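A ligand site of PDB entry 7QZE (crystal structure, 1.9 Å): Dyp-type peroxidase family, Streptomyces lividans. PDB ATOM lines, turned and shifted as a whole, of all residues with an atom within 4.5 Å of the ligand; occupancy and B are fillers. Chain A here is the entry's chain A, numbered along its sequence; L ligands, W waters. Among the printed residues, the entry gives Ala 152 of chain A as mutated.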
ATOM      1  N   ASP A 146       9.417  18.357  29.382  1.00  0.00           N
ATOM      2  CA  ASP A 146       8.429  17.751  28.460  1.00  0.00           C
ATOM      3  C   ASP A 146       9.120  16.620  27.709  1.00  0.00           C
ATOM      4  O   ASP A 146      10.348  16.395  27.911  1.00  0.00           O
ATOM      5  CB  ASP A 146       7.769  18.816  27.581  1.00  0.00           C
ATOM      6  CG  ASP A 146       8.715  19.549  26.649  1.00  0.00           C
ATOM      7  OD1 ASP A 146       9.866  19.059  26.416  1.00  0.00           O
ATOM      8  OD2 ASP A 146       8.315  20.639  26.224  1.00  0.00           O
ATOM      9  N   LEU A 148       9.985  16.585  24.749  1.00  0.00           N
ATOM     10  CA  LEU A 148      11.063  17.068  23.850  1.00  0.00           C
ATOM     11  C   LEU A 148      12.388  17.282  24.592  1.00  0.00           C
ATOM     12  O   LEU A 148      13.389  17.608  23.893  1.00  0.00           O
ATOM     13  CB  LEU A 148      10.597  18.335  23.118  1.00  0.00           C
ATOM     14  CG  LEU A 148       9.283  18.176  22.358  1.00  0.00           C
ATOM     15  CD1 LEU A 148       8.928  19.482  21.659  1.00  0.00           C
ATOM     16  CD2 LEU A 148       9.381  17.059  21.334  1.00  0.00           C
ATOM     17  N   PHE A 150      12.882  19.651  27.043  1.00  0.00           N
ATOM     18  CA  PHE A 150      13.003  21.073  27.456  1.00  0.00           C
ATOM     19  C   PHE A 150      12.160  21.282  28.699  1.00  0.00           C
ATOM     20  O   PHE A 150      11.091  20.636  28.838  1.00  0.00           O
ATOM     21  CB  PHE A 150      12.551  22.037  26.351  1.00  0.00           C
ATOM     22  CG  PHE A 150      13.582  22.236  25.274  1.00  0.00           C
ATOM     23  CD1 PHE A 150      13.898  21.208  24.389  1.00  0.00           C
ATOM     24  CD2 PHE A 150      14.271  23.435  25.156  1.00  0.00           C
ATOM     25  CE1 PHE A 150      14.871  21.364  23.422  1.00  0.00           C
ATOM     26  CE2 PHE A 150      15.237  23.584  24.174  1.00  0.00           C
ATOM     27  CZ  PHE A 150      15.528  22.565  23.303  1.00  0.00           C
ATOM     28  N   VAL A 151      12.594  22.208  29.546  1.00  0.00           N
ATOM     29  CA  VAL A 151      11.826  22.623  30.756  1.00  0.00           C
ATOM     30  C   VAL A 151      10.576  23.337  30.261  1.00  0.00           C
ATOM     31  O   VAL A 151      10.696  24.159  29.347  1.00  0.00           O
ATOM     32  CB  VAL A 151      12.658  23.496  31.717  1.00  0.00           C
ATOM     33  CG1 VAL A 151      11.882  23.933  32.947  1.00  0.00           C
ATOM     34  CG2 VAL A 151      13.931  22.761  32.147  1.00  0.00           C
ATOM     35  N   ALA A 152       9.424  23.020  30.848  1.00  0.00           N
ATOM     36  CA  ALA A 152       8.135  23.595  30.409  1.00  0.00           C
ATOM     37  C   ALA A 152       7.433  24.234  31.615  1.00  0.00           C
ATOM     38  O   ALA A 152       7.224  23.526  32.623  1.00  0.00           O
ATOM     39  CB  ALA A 152       7.278  22.548  29.741  1.00  0.00           C
ATOM     40  N   GLY A 153       7.137  25.531  31.522  1.00  0.00           N
ATOM     41  CA  GLY A 153       6.362  26.314  32.516  1.00  0.00           C
ATOM     42  C   GLY A 153       7.123  27.538  33.009  1.00  0.00           C
ATOM     43  O   GLY A 153       6.523  28.345  33.756  1.00  0.00           O
ATOM     44  N   THR A 154       8.408  27.668  32.639  1.00  0.00           N
ATOM     45  CA  THR A 154       9.353  28.664  33.199  1.00  0.00           C
ATOM     46  C   THR A 154       8.737  30.083  33.215  1.00  0.00           C
ATOM     47  O   THR A 154       8.798  30.694  34.253  1.00  0.00           O
ATOM     48  CB  THR A 154      10.646  28.670  32.385  1.00  0.00           C
ATOM     49  OG1 THR A 154      11.115  27.339  32.260  1.00  0.00           O
ATOM     50  CG2 THR A 154      11.742  29.495  33.016  1.00  0.00           C
ATOM     51  N   GLU A 155       8.163  30.564  32.101  1.00  0.00           N
ATOM     52  CA  GLU A 155       7.693  31.978  31.966  1.00  0.00           C
ATOM     53  C   GLU A 155       6.207  32.108  32.338  1.00  0.00           C
ATOM     54  O   GLU A 155       5.633  33.174  32.082  1.00  0.00           O
ATOM     55  CB  GLU A 155       8.030  32.489  30.574  1.00  0.00           C
ATOM     56  CG  GLU A 155       9.509  32.672  30.359  1.00  0.00           C
ATOM     57  CD  GLU A 155      10.059  33.709  31.308  1.00  0.00           C
ATOM     58  OE1 GLU A 155       9.588  34.843  31.241  1.00  0.00           O
ATOM     59  OE2 GLU A 155      10.870  33.352  32.170  1.00  0.00           O
ATOM     60  N   GLN A 184      -5.447  21.059  24.335  1.00  0.00           N
ATOM     61  CA  GLN A 184      -5.065  20.339  23.111  1.00  0.00           C
ATOM     62  C   GLN A 184      -4.153  19.189  23.509  1.00  0.00           C
ATOM     63  O   GLN A 184      -3.080  19.460  24.123  1.00  0.00           O
ATOM     64  CB  GLN A 184      -4.296  21.272  22.177  1.00  0.00           C
ATOM     65  CG  GLN A 184      -5.143  22.394  21.581  1.00  0.00           C
ATOM     66  CD  GLN A 184      -4.235  23.156  20.661  1.00  0.00           C
ATOM     67  OE1 GLN A 184      -3.208  23.714  21.088  1.00  0.00           O
ATOM     68  NE2 GLN A 184      -4.561  23.127  19.375  1.00  0.00           N
ATOM     69  N   TYR A 186      -1.364  16.799  22.328  1.00  0.00           N
ATOM     70  CA  TYR A 186      -0.309  16.800  21.303  1.00  0.00           C
ATOM     71  C   TYR A 186       0.449  15.484  21.374  1.00  0.00           C
ATOM     72  O   TYR A 186       0.732  15.057  22.490  1.00  0.00           O
ATOM     73  CB  TYR A 186       0.665  17.963  21.489  1.00  0.00           C
ATOM     74  CG  TYR A 186       0.161  19.289  21.003  1.00  0.00           C
ATOM     75  CD1 TYR A 186       0.300  19.666  19.684  1.00  0.00           C
ATOM     76  CD2 TYR A 186      -0.424  20.179  21.879  1.00  0.00           C
ATOM     77  CE1 TYR A 186      -0.107  20.904  19.227  1.00  0.00           C
ATOM     78  CE2 TYR A 186      -0.836  21.430  21.439  1.00  0.00           C
ATOM     79  CZ  TYR A 186      -0.700  21.775  20.115  1.00  0.00           C
ATOM     80  OH  TYR A 186      -1.103  22.986  19.669  1.00  0.00           O
ATOM     81  N   HIS A 188       4.032  13.770  19.769  1.00  0.00           N
ATOM     82  CA  HIS A 188       5.317  14.245  19.240  1.00  0.00           C
ATOM     83  C   HIS A 188       5.917  13.151  18.348  1.00  0.00           C
ATOM     84  O   HIS A 188       5.847  11.975  18.724  1.00  0.00           O
ATOM     85  CB  HIS A 188       6.285  14.622  20.352  1.00  0.00           C
ATOM     86  CG  HIS A 188       5.807  15.770  21.175  1.00  0.00           C
ATOM     87  ND1 HIS A 188       5.666  17.027  20.640  1.00  0.00           N
ATOM     88  CD2 HIS A 188       5.478  15.851  22.490  1.00  0.00           C
ATOM     89  CE1 HIS A 188       5.211  17.842  21.585  1.00  0.00           C
ATOM     90  NE2 HIS A 188       5.072  17.150  22.725  1.00  0.00           N
ATOM     91  N   ILE A 205      12.758  25.906  19.827  1.00  0.00           N
ATOM     92  CA  ILE A 205      12.085  26.321  21.096  1.00  0.00           C
ATOM     93  C   ILE A 205      12.329  27.810  21.336  1.00  0.00           C
ATOM     94  O   ILE A 205      11.343  28.523  21.604  1.00  0.00           O
ATOM     95  CB  ILE A 205      12.524  25.449  22.287  1.00  0.00           C
ATOM     96  CG1 ILE A 205      12.269  23.954  22.054  1.00  0.00           C
ATOM     97  CG2 ILE A 205      11.869  25.964  23.570  1.00  0.00           C
ATOM     98  CD1 ILE A 205      10.810  23.567  21.933  1.00  0.00           C
ATOM     99  N   ARG A 207      14.978  28.633  23.601  1.00  0.00           N
ATOM    100  CA  ARG A 207      15.696  28.561  24.901  1.00  0.00           C
ATOM    101  C   ARG A 207      16.804  27.515  24.792  1.00  0.00           C
ATOM    102  O   ARG A 207      16.647  26.570  23.981  1.00  0.00           O
ATOM    103  CB  ARG A 207      14.755  28.224  26.062  1.00  0.00           C
ATOM    104  CG  ARG A 207      13.477  29.045  26.113  1.00  0.00           C
ATOM    105  CD  ARG A 207      12.609  28.780  27.310  1.00  0.00           C
ATOM    106  NE  ARG A 207      13.232  29.251  28.528  1.00  0.00           N
ATOM    107  CZ  ARG A 207      13.102  30.479  29.039  1.00  0.00           C
ATOM    108  NH1 ARG A 207      12.275  31.361  28.509  1.00  0.00           N
ATOM    109  NH2 ARG A 207      13.767  30.797  30.121  1.00  0.00           N
ATOM    110  N   HIS A 225       9.220  28.790  19.009  1.00  0.00           N
ATOM    111  CA  HIS A 225       8.005  28.729  19.867  1.00  0.00           C
ATOM    112  C   HIS A 225       7.901  29.954  20.775  1.00  0.00           C
ATOM    113  O   HIS A 225       6.794  30.583  20.855  1.00  0.00           O
ATOM    114  CB  HIS A 225       8.041  27.445  20.672  1.00  0.00           C
ATOM    115  CG  HIS A 225       6.808  27.231  21.458  1.00  0.00           C
ATOM    116  ND1 HIS A 225       5.582  27.181  20.863  1.00  0.00           N
ATOM    117  CD2 HIS A 225       6.635  26.978  22.757  1.00  0.00           C
ATOM    118  CE1 HIS A 225       4.668  26.929  21.777  1.00  0.00           C
ATOM    119  NE2 HIS A 225       5.295  26.787  22.952  1.00  0.00           N
ATOM    120  N   VAL A 226       8.989  30.300  21.458  1.00  0.00           N
ATOM    121  CA  VAL A 226       8.998  31.470  22.380  1.00  0.00           C
ATOM    122  C   VAL A 226       8.677  32.766  21.600  1.00  0.00           C
ATOM    123  O   VAL A 226       7.864  33.563  22.113  1.00  0.00           O
ATOM    124  CB  VAL A 226      10.287  31.562  23.196  1.00  0.00           C
ATOM    125  CG1 VAL A 226      10.400  32.902  23.935  1.00  0.00           C
ATOM    126  CG2 VAL A 226      10.361  30.389  24.153  1.00  0.00           C
ATOM    127  N   THR A 229       4.802  32.818  20.596  1.00  0.00           N
ATOM    128  CA  THR A 229       3.850  32.798  21.727  1.00  0.00           C
ATOM    129  C   THR A 229       4.036  34.035  22.610  1.00  0.00           C
ATOM    130  O   THR A 229       3.325  34.128  23.616  1.00  0.00           O
ATOM    131  CB  THR A 229       3.887  31.480  22.506  1.00  0.00           C
ATOM    132  OG1 THR A 229       5.206  31.265  22.992  1.00  0.00           O
ATOM    133  CG2 THR A 229       3.445  30.305  21.652  1.00  0.00           C
ATOM    134  N   SER A 230       5.003  34.893  22.289  1.00  0.00           N
ATOM    135  CA  SER A 230       5.225  36.210  22.946  1.00  0.00           C
ATOM    136  C   SER A 230       4.327  37.248  22.253  1.00  0.00           C
ATOM    137  O   SER A 230       4.545  37.473  21.043  1.00  0.00           O
ATOM    138  CB  SER A 230       6.678  36.626  22.849  1.00  0.00           C
ATOM    139  OG  SER A 230       7.457  35.722  23.598  1.00  0.00           O
ATOM    140  N   ILE A 241      -0.692  33.892  29.450  1.00  0.00           N
ATOM    141  CA  ILE A 241      -1.587  32.796  29.916  1.00  0.00           C
ATOM    142  C   ILE A 241      -0.876  31.980  31.002  1.00  0.00           C
ATOM    143  O   ILE A 241       0.338  32.082  31.101  1.00  0.00           O
ATOM    144  CB  ILE A 241      -2.018  31.958  28.701  1.00  0.00           C
ATOM    145  CG1 ILE A 241      -0.858  31.217  28.052  1.00  0.00           C
ATOM    146  CG2 ILE A 241      -2.754  32.831  27.696  1.00  0.00           C
ATOM    147  CD1 ILE A 241      -1.344  30.182  27.085  1.00  0.00           C
ATOM    148  N   ARG A 243      -0.089  28.102  31.967  1.00  0.00           N
ATOM    149  CA  ARG A 243      -0.031  26.762  31.334  1.00  0.00           C
ATOM    150  C   ARG A 243       0.288  25.723  32.398  1.00  0.00           C
ATOM    151  O   ARG A 243       1.189  25.964  33.245  1.00  0.00           O
ATOM    152  CB  ARG A 243       1.037  26.754  30.239  1.00  0.00           C
ATOM    153  CG  ARG A 243       0.714  27.612  29.046  1.00  0.00           C
ATOM    154  CD  ARG A 243       1.912  27.902  28.173  1.00  0.00           C
ATOM    155  NE  ARG A 243       2.911  28.671  28.916  1.00  0.00           N
ATOM    156  CZ  ARG A 243       4.166  28.285  29.166  1.00  0.00           C
ATOM    157  NH1 ARG A 243       4.625  27.116  28.729  1.00  0.00           N
ATOM    158  NH2 ARG A 243       4.981  29.082  29.860  1.00  0.00           N
ATOM    159  N   ASN A 245       0.855  22.328  31.437  1.00  0.00           N
ATOM    160  CA  ASN A 245       1.211  21.238  30.513  1.00  0.00           C
ATOM    161  C   ASN A 245       1.740  20.036  31.290  1.00  0.00           C
ATOM    162  O   ASN A 245       2.578  20.211  32.170  1.00  0.00           O
ATOM    163  CB  ASN A 245       2.262  21.687  29.498  1.00  0.00           C
ATOM    164  CG  ASN A 245       1.792  22.827  28.618  1.00  0.00           C
ATOM    165  OD1 ASN A 245       0.732  23.427  28.841  1.00  0.00           O
ATOM    166  ND2 ASN A 245       2.574  23.133  27.602  1.00  0.00           N
ATOM    167  N   THR A 258       2.433  15.702  24.862  1.00  0.00           N
ATOM    168  CA  THR A 258       2.252  16.864  25.760  1.00  0.00           C
ATOM    169  C   THR A 258       0.745  17.145  25.837  1.00  0.00           C
ATOM    170  O   THR A 258       0.112  17.379  24.782  1.00  0.00           O
ATOM    171  CB  THR A 258       2.959  18.106  25.232  1.00  0.00           C
ATOM    172  OG1 THR A 258       4.367  17.826  25.195  1.00  0.00           O
ATOM    173  CG2 THR A 258       2.638  19.341  26.059  1.00  0.00           C
ATOM    174  N   PHE A 260      -1.537  19.925  26.570  1.00  0.00           N
ATOM    175  CA  PHE A 260      -1.556  21.405  26.718  1.00  0.00           C
ATOM    176  C   PHE A 260      -2.853  21.836  27.415  1.00  0.00           C
ATOM    177  O   PHE A 260      -3.947  21.430  27.013  1.00  0.00           O
ATOM    178  CB  PHE A 260      -1.467  22.094  25.354  1.00  0.00           C
ATOM    179  CG  PHE A 260      -1.659  23.587  25.467  1.00  0.00           C
ATOM    180  CD1 PHE A 260      -0.638  24.384  25.938  1.00  0.00           C
ATOM    181  CD2 PHE A 260      -2.883  24.162  25.219  1.00  0.00           C
ATOM    182  CE1 PHE A 260      -0.808  25.751  26.093  1.00  0.00           C
ATOM    183  CE2 PHE A 260      -3.064  25.527  25.372  1.00  0.00           C
ATOM    184  CZ  PHE A 260      -2.026  26.321  25.809  1.00  0.00           C
ATOM    185  N   THR A 270      -5.319  33.460  24.257  1.00  0.00           N
ATOM    186  CA  THR A 270      -4.920  32.076  23.905  1.00  0.00           C
ATOM    187  C   THR A 270      -5.102  31.861  22.395  1.00  0.00           C
ATOM    188  O   THR A 270      -4.224  31.268  21.770  1.00  0.00           O
ATOM    189  CB  THR A 270      -5.734  31.058  24.699  1.00  0.00           C
ATOM    190  OG1 THR A 270      -5.728  31.409  26.077  1.00  0.00           O
ATOM    191  CG2 THR A 270      -5.201  29.660  24.512  1.00  0.00           C
ATOM    192  N   MET A 273      -2.415  33.548  20.283  1.00  0.00           N
ATOM    193  CA  MET A 273      -1.201  32.682  20.318  1.00  0.00           C
ATOM    194  C   MET A 273      -1.346  31.516  19.327  1.00  0.00           C
ATOM    195  O   MET A 273      -0.385  31.267  18.546  1.00  0.00           O
ATOM    196  CB  MET A 273      -0.950  32.157  21.729  1.00  0.00           C
ATOM    197  CG  MET A 273      -0.465  33.239  22.641  1.00  0.00           C
ATOM    198  SD  MET A 273      -0.325  32.658  24.331  1.00  0.00           S
ATOM    199  CE  MET A 273       0.464  34.104  25.027  1.00  0.00           C
ATOM    200  N   LEU A 274      -2.486  30.850  19.343  1.00  0.00           N
ATOM    201  CA  LEU A 274      -2.761  29.694  18.450  1.00  0.00           C
ATOM    202  C   LEU A 274      -2.756  30.127  16.974  1.00  0.00           C
ATOM    203  O   LEU A 274      -2.149  29.391  16.149  1.00  0.00           O
ATOM    204  CB  LEU A 274      -4.101  29.082  18.847  1.00  0.00           C
ATOM    205  CG  LEU A 274      -4.051  28.144  20.046  1.00  0.00           C
ATOM    206  CD1 LEU A 274      -5.441  27.732  20.423  1.00  0.00           C
ATOM    207  CD2 LEU A 274      -3.198  26.913  19.763  1.00  0.00           C
ATOM    208  N   MET A 277       0.816  30.516  15.896  1.00  0.00           N
ATOM    209  CA  MET A 277       1.475  29.186  15.812  1.00  0.00           C
ATOM    210  C   MET A 277       1.076  28.501  14.504  1.00  0.00           C
ATOM    211  O   MET A 277       1.974  28.042  13.822  1.00  0.00           O
ATOM    212  CB  MET A 277       1.109  28.275  16.995  1.00  0.00           C
ATOM    213  CG  MET A 277       1.742  28.726  18.314  1.00  0.00           C
ATOM    214  SD  MET A 277       1.201  27.737  19.685  1.00  0.00           S
ATOM    215  CE  MET A 277       1.739  26.109  19.159  1.00  0.00           C
ATOM    216  N   ILE A 289       7.763  24.263  16.351  1.00  0.00           N
ATOM    217  CA  ILE A 289       7.416  23.142  17.282  1.00  0.00           C
ATOM    218  C   ILE A 289       6.334  22.256  16.646  1.00  0.00           C
ATOM    219  O   ILE A 289       6.343  21.031  16.904  1.00  0.00           O
ATOM    220  CB  ILE A 289       7.019  23.684  18.666  1.00  0.00           C
ATOM    221  CG1 ILE A 289       7.463  22.713  19.756  1.00  0.00           C
ATOM    222  CG2 ILE A 289       5.515  23.997  18.747  1.00  0.00           C
ATOM    223  CD1 ILE A 289       7.237  23.209  21.170  1.00  0.00           C
ATOM    224  N   SER A 293       5.073  18.055  16.312  1.00  0.00           N
ATOM    225  CA  SER A 293       3.954  17.968  17.262  1.00  0.00           C
ATOM    226  C   SER A 293       2.629  18.013  16.496  1.00  0.00           C
ATOM    227  O   SER A 293       2.405  18.994  15.796  1.00  0.00           O
ATOM    228  CB  SER A 293       4.046  19.074  18.278  1.00  0.00           C
ATOM    229  OG  SER A 293       5.380  19.232  18.751  1.00  0.00           O
HETATM  230  C1  LIG L   1       6.725  28.399  26.348  1.00  0.00           C
HETATM  231  C2  LIG L   1       6.651  23.684  25.131  1.00  0.00           C
HETATM  232  C3  LIG L   1       2.219  24.271  23.105  1.00  0.00           C
HETATM  233  C4  LIG L   1       2.157  28.791  24.767  1.00  0.00           C
HETATM  234  C5  LIG L   1       7.070  27.066  26.151  1.00  0.00           C
HETATM  235  C6  LIG L   1       8.361  26.546  26.494  1.00  0.00           C
HETATM  236  C7  LIG L   1       8.307  25.210  26.134  1.00  0.00           C
HETATM  237  C8  LIG L   1       7.032  24.915  25.599  1.00  0.00           C
HETATM  238  C9  LIG L   1       9.389  24.173  26.338  1.00  0.00           C
HETATM  239  C10 LIG L   1       9.536  27.321  27.083  1.00  0.00           C
HETATM  240  C11 LIG L   1       9.550  27.430  28.625  1.00  0.00           C
HETATM  241  C12 LIG L   1       8.266  28.015  29.217  1.00  0.00           C
HETATM  242  O1  LIG L   1       7.266  27.291  29.422  1.00  0.00           O
HETATM  243  O2  LIG L   1       8.228  29.230  29.462  1.00  0.00           O
HETATM  244  C13 LIG L   1       5.433  23.458  24.454  1.00  0.00           C
HETATM  245  C14 LIG L   1       5.116  22.185  23.892  1.00  0.00           C
HETATM  246  C15 LIG L   1       3.861  22.295  23.326  1.00  0.00           C
HETATM  247  C16 LIG L   1       3.422  23.719  23.539  1.00  0.00           C
HETATM  248  C17 LIG L   1       5.998  20.959  23.966  1.00  0.00           C
HETATM  249  C18 LIG L   1       3.283  21.232  22.540  1.00  0.00           C
HETATM  250  C19 LIG L   1       2.691  21.526  21.404  1.00  0.00           C
HETATM  251  C20 LIG L   1       1.798  25.568  23.382  1.00  0.00           C
HETATM  252  C21 LIG L   1       0.563  26.161  22.964  1.00  0.00           C
HETATM  253  C22 LIG L   1       0.561  27.466  23.407  1.00  0.00           C
HETATM  254  C23 LIG L   1       1.803  27.640  24.138  1.00  0.00           C
HETATM  255  C24 LIG L   1      -0.492  25.429  22.202  1.00  0.00           C
HETATM  256  C25 LIG L   1      -0.415  28.565  23.380  1.00  0.00           C
HETATM  257  C26 LIG L   1      -1.628  28.452  22.933  1.00  0.00           C
HETATM  258  C27 LIG L   1       3.423  29.017  25.324  1.00  0.00           C
HETATM  259  C28 LIG L   1       3.771  30.312  25.931  1.00  0.00           C
HETATM  260  C29 LIG L   1       5.031  30.223  26.353  1.00  0.00           C
HETATM  261  C30 LIG L   1       5.454  28.864  26.014  1.00  0.00           C
HETATM  262  C31 LIG L   1       2.899  31.520  26.103  1.00  0.00           C
HETATM  263  C32 LIG L   1       5.786  31.300  27.042  1.00  0.00           C
HETATM  264  C33 LIG L   1       6.560  32.088  26.007  1.00  0.00           C
HETATM  265  C34 LIG L   1       7.255  33.253  26.690  1.00  0.00           C
HETATM  266  O3  LIG L   1       6.614  34.310  26.989  1.00  0.00           O
HETATM  267  O4  LIG L   1       8.471  33.156  26.929  1.00  0.00           O
HETATM  268  N1  LIG L   1       6.271  26.038  25.626  1.00  0.00           N
HETATM  269  N2  LIG L   1       4.403  24.312  24.234  1.00  0.00           N
HETATM  270  N3  LIG L   1       2.516  26.478  24.068  1.00  0.00           N
HETATM  271  N4  LIG L   1       4.439  28.172  25.415  1.00  0.00           N
HETATM  272 FE1  LIG L   1       4.437  26.301  24.842  1.00  0.00          FE
HETATM  273  O   HOH W   1       9.716  30.855  27.523  1.00  0.00           O
HETATM  274  O   HOH W   2       7.539  36.826  26.634  1.00  0.00           O
HETATM  275  O   HOH W   3       3.934  34.566  26.496  1.00  0.00           O
HETATM  276  O   HOH W   4       5.297  21.308  27.333  1.00  0.00           O
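Residues that only touch the ligand: Asp 146, Phe 150, Val 151, Ala 152, Gln 184, Tyr 186, Arg 207, Val 226, Thr 229, Ser 230, Thr 258, Phe 260, Met 273, Leu 274, Met 277 and Ile 289. Hydrophobic or aromatic side chains that line the ligand: Phe 150, Tyr 186, His 225, Val 226, Phe 260, Met 273, Leu 274, Met 277 and Ile 289. Along chain A the residues within 4 Å of the ligand span positions 146 to 289. The nearest printed residue that does not touch the ligand is His 188 (4.001 Å).
Water W1 lies within hydrogen-bond range of an oxygen (O4) of the ligand (2.7 Å) and the guanidinium group (NH1) of Arg 207 (2.8 Å). Water W2 lies within hydrogen-bond range of O3 of the ligand (2.7 Å) and OG of Ser 230 (3.2 Å). Water W3 lies within hydrogen-bond range of an oxygen (O3) of the ligand and the backbone carbonyl oxygen (O) of Thr 229. Water W4 lies within hydrogen-bond range of OD2 of Asp 146 (3.3 Å) and ND2 of Asn 245 (3.3 Å).
The backbone carbonyl oxygen of His 225 sits at hydrogen-bond distance from the side-chain hydroxyl of Thr 229 (2.7 Å). OD1 of Asp 146 lies within hydrogen-bond range of N of Leu 148, 3.0 Å away. The side-chain hydroxyl (OH) of Tyr 186 sits at hydrogen-bond distance from the side-chain amide oxygen (OE1) of Gln 184 (2.6 Å). O of Gln 184 sits at hydrogen-bond distance from N of Phe 260. N of Tyr 186 lies within hydrogen-bond range of O of Thr 258 (2.9 Å). N of Val 226 lies within hydrogen-bond range of O of Ile 205 (3.0 Å). OG of Ser 293 is in hydrogen-bond range of O of Ile 289 (2.8 Å). OG1 of Thr 258 lies within hydrogen-bond range of NE2 of His 188.
A ring nitrogen (NE2) of His 225 binds an iron atom (FE1) of the ligand (2.1 Å). An oxygen (O1) of the ligand is in salt-bridge range of the guanidinium group (NH1) of Arg 243 (2.7 Å). The backbone NH of Gly 153 lies within hydrogen-bond range of an oxygen (O1) of the ligand, at 2.7 Å. The backbone NH of Glu 155 sits at hydrogen-bond distance from an oxygen (O2) of the ligand (3.0 Å). The backbone NH (N) of Thr 154 lies within hydrogen-bond range of an oxygen (O1) of the ligand (3.4 Å).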
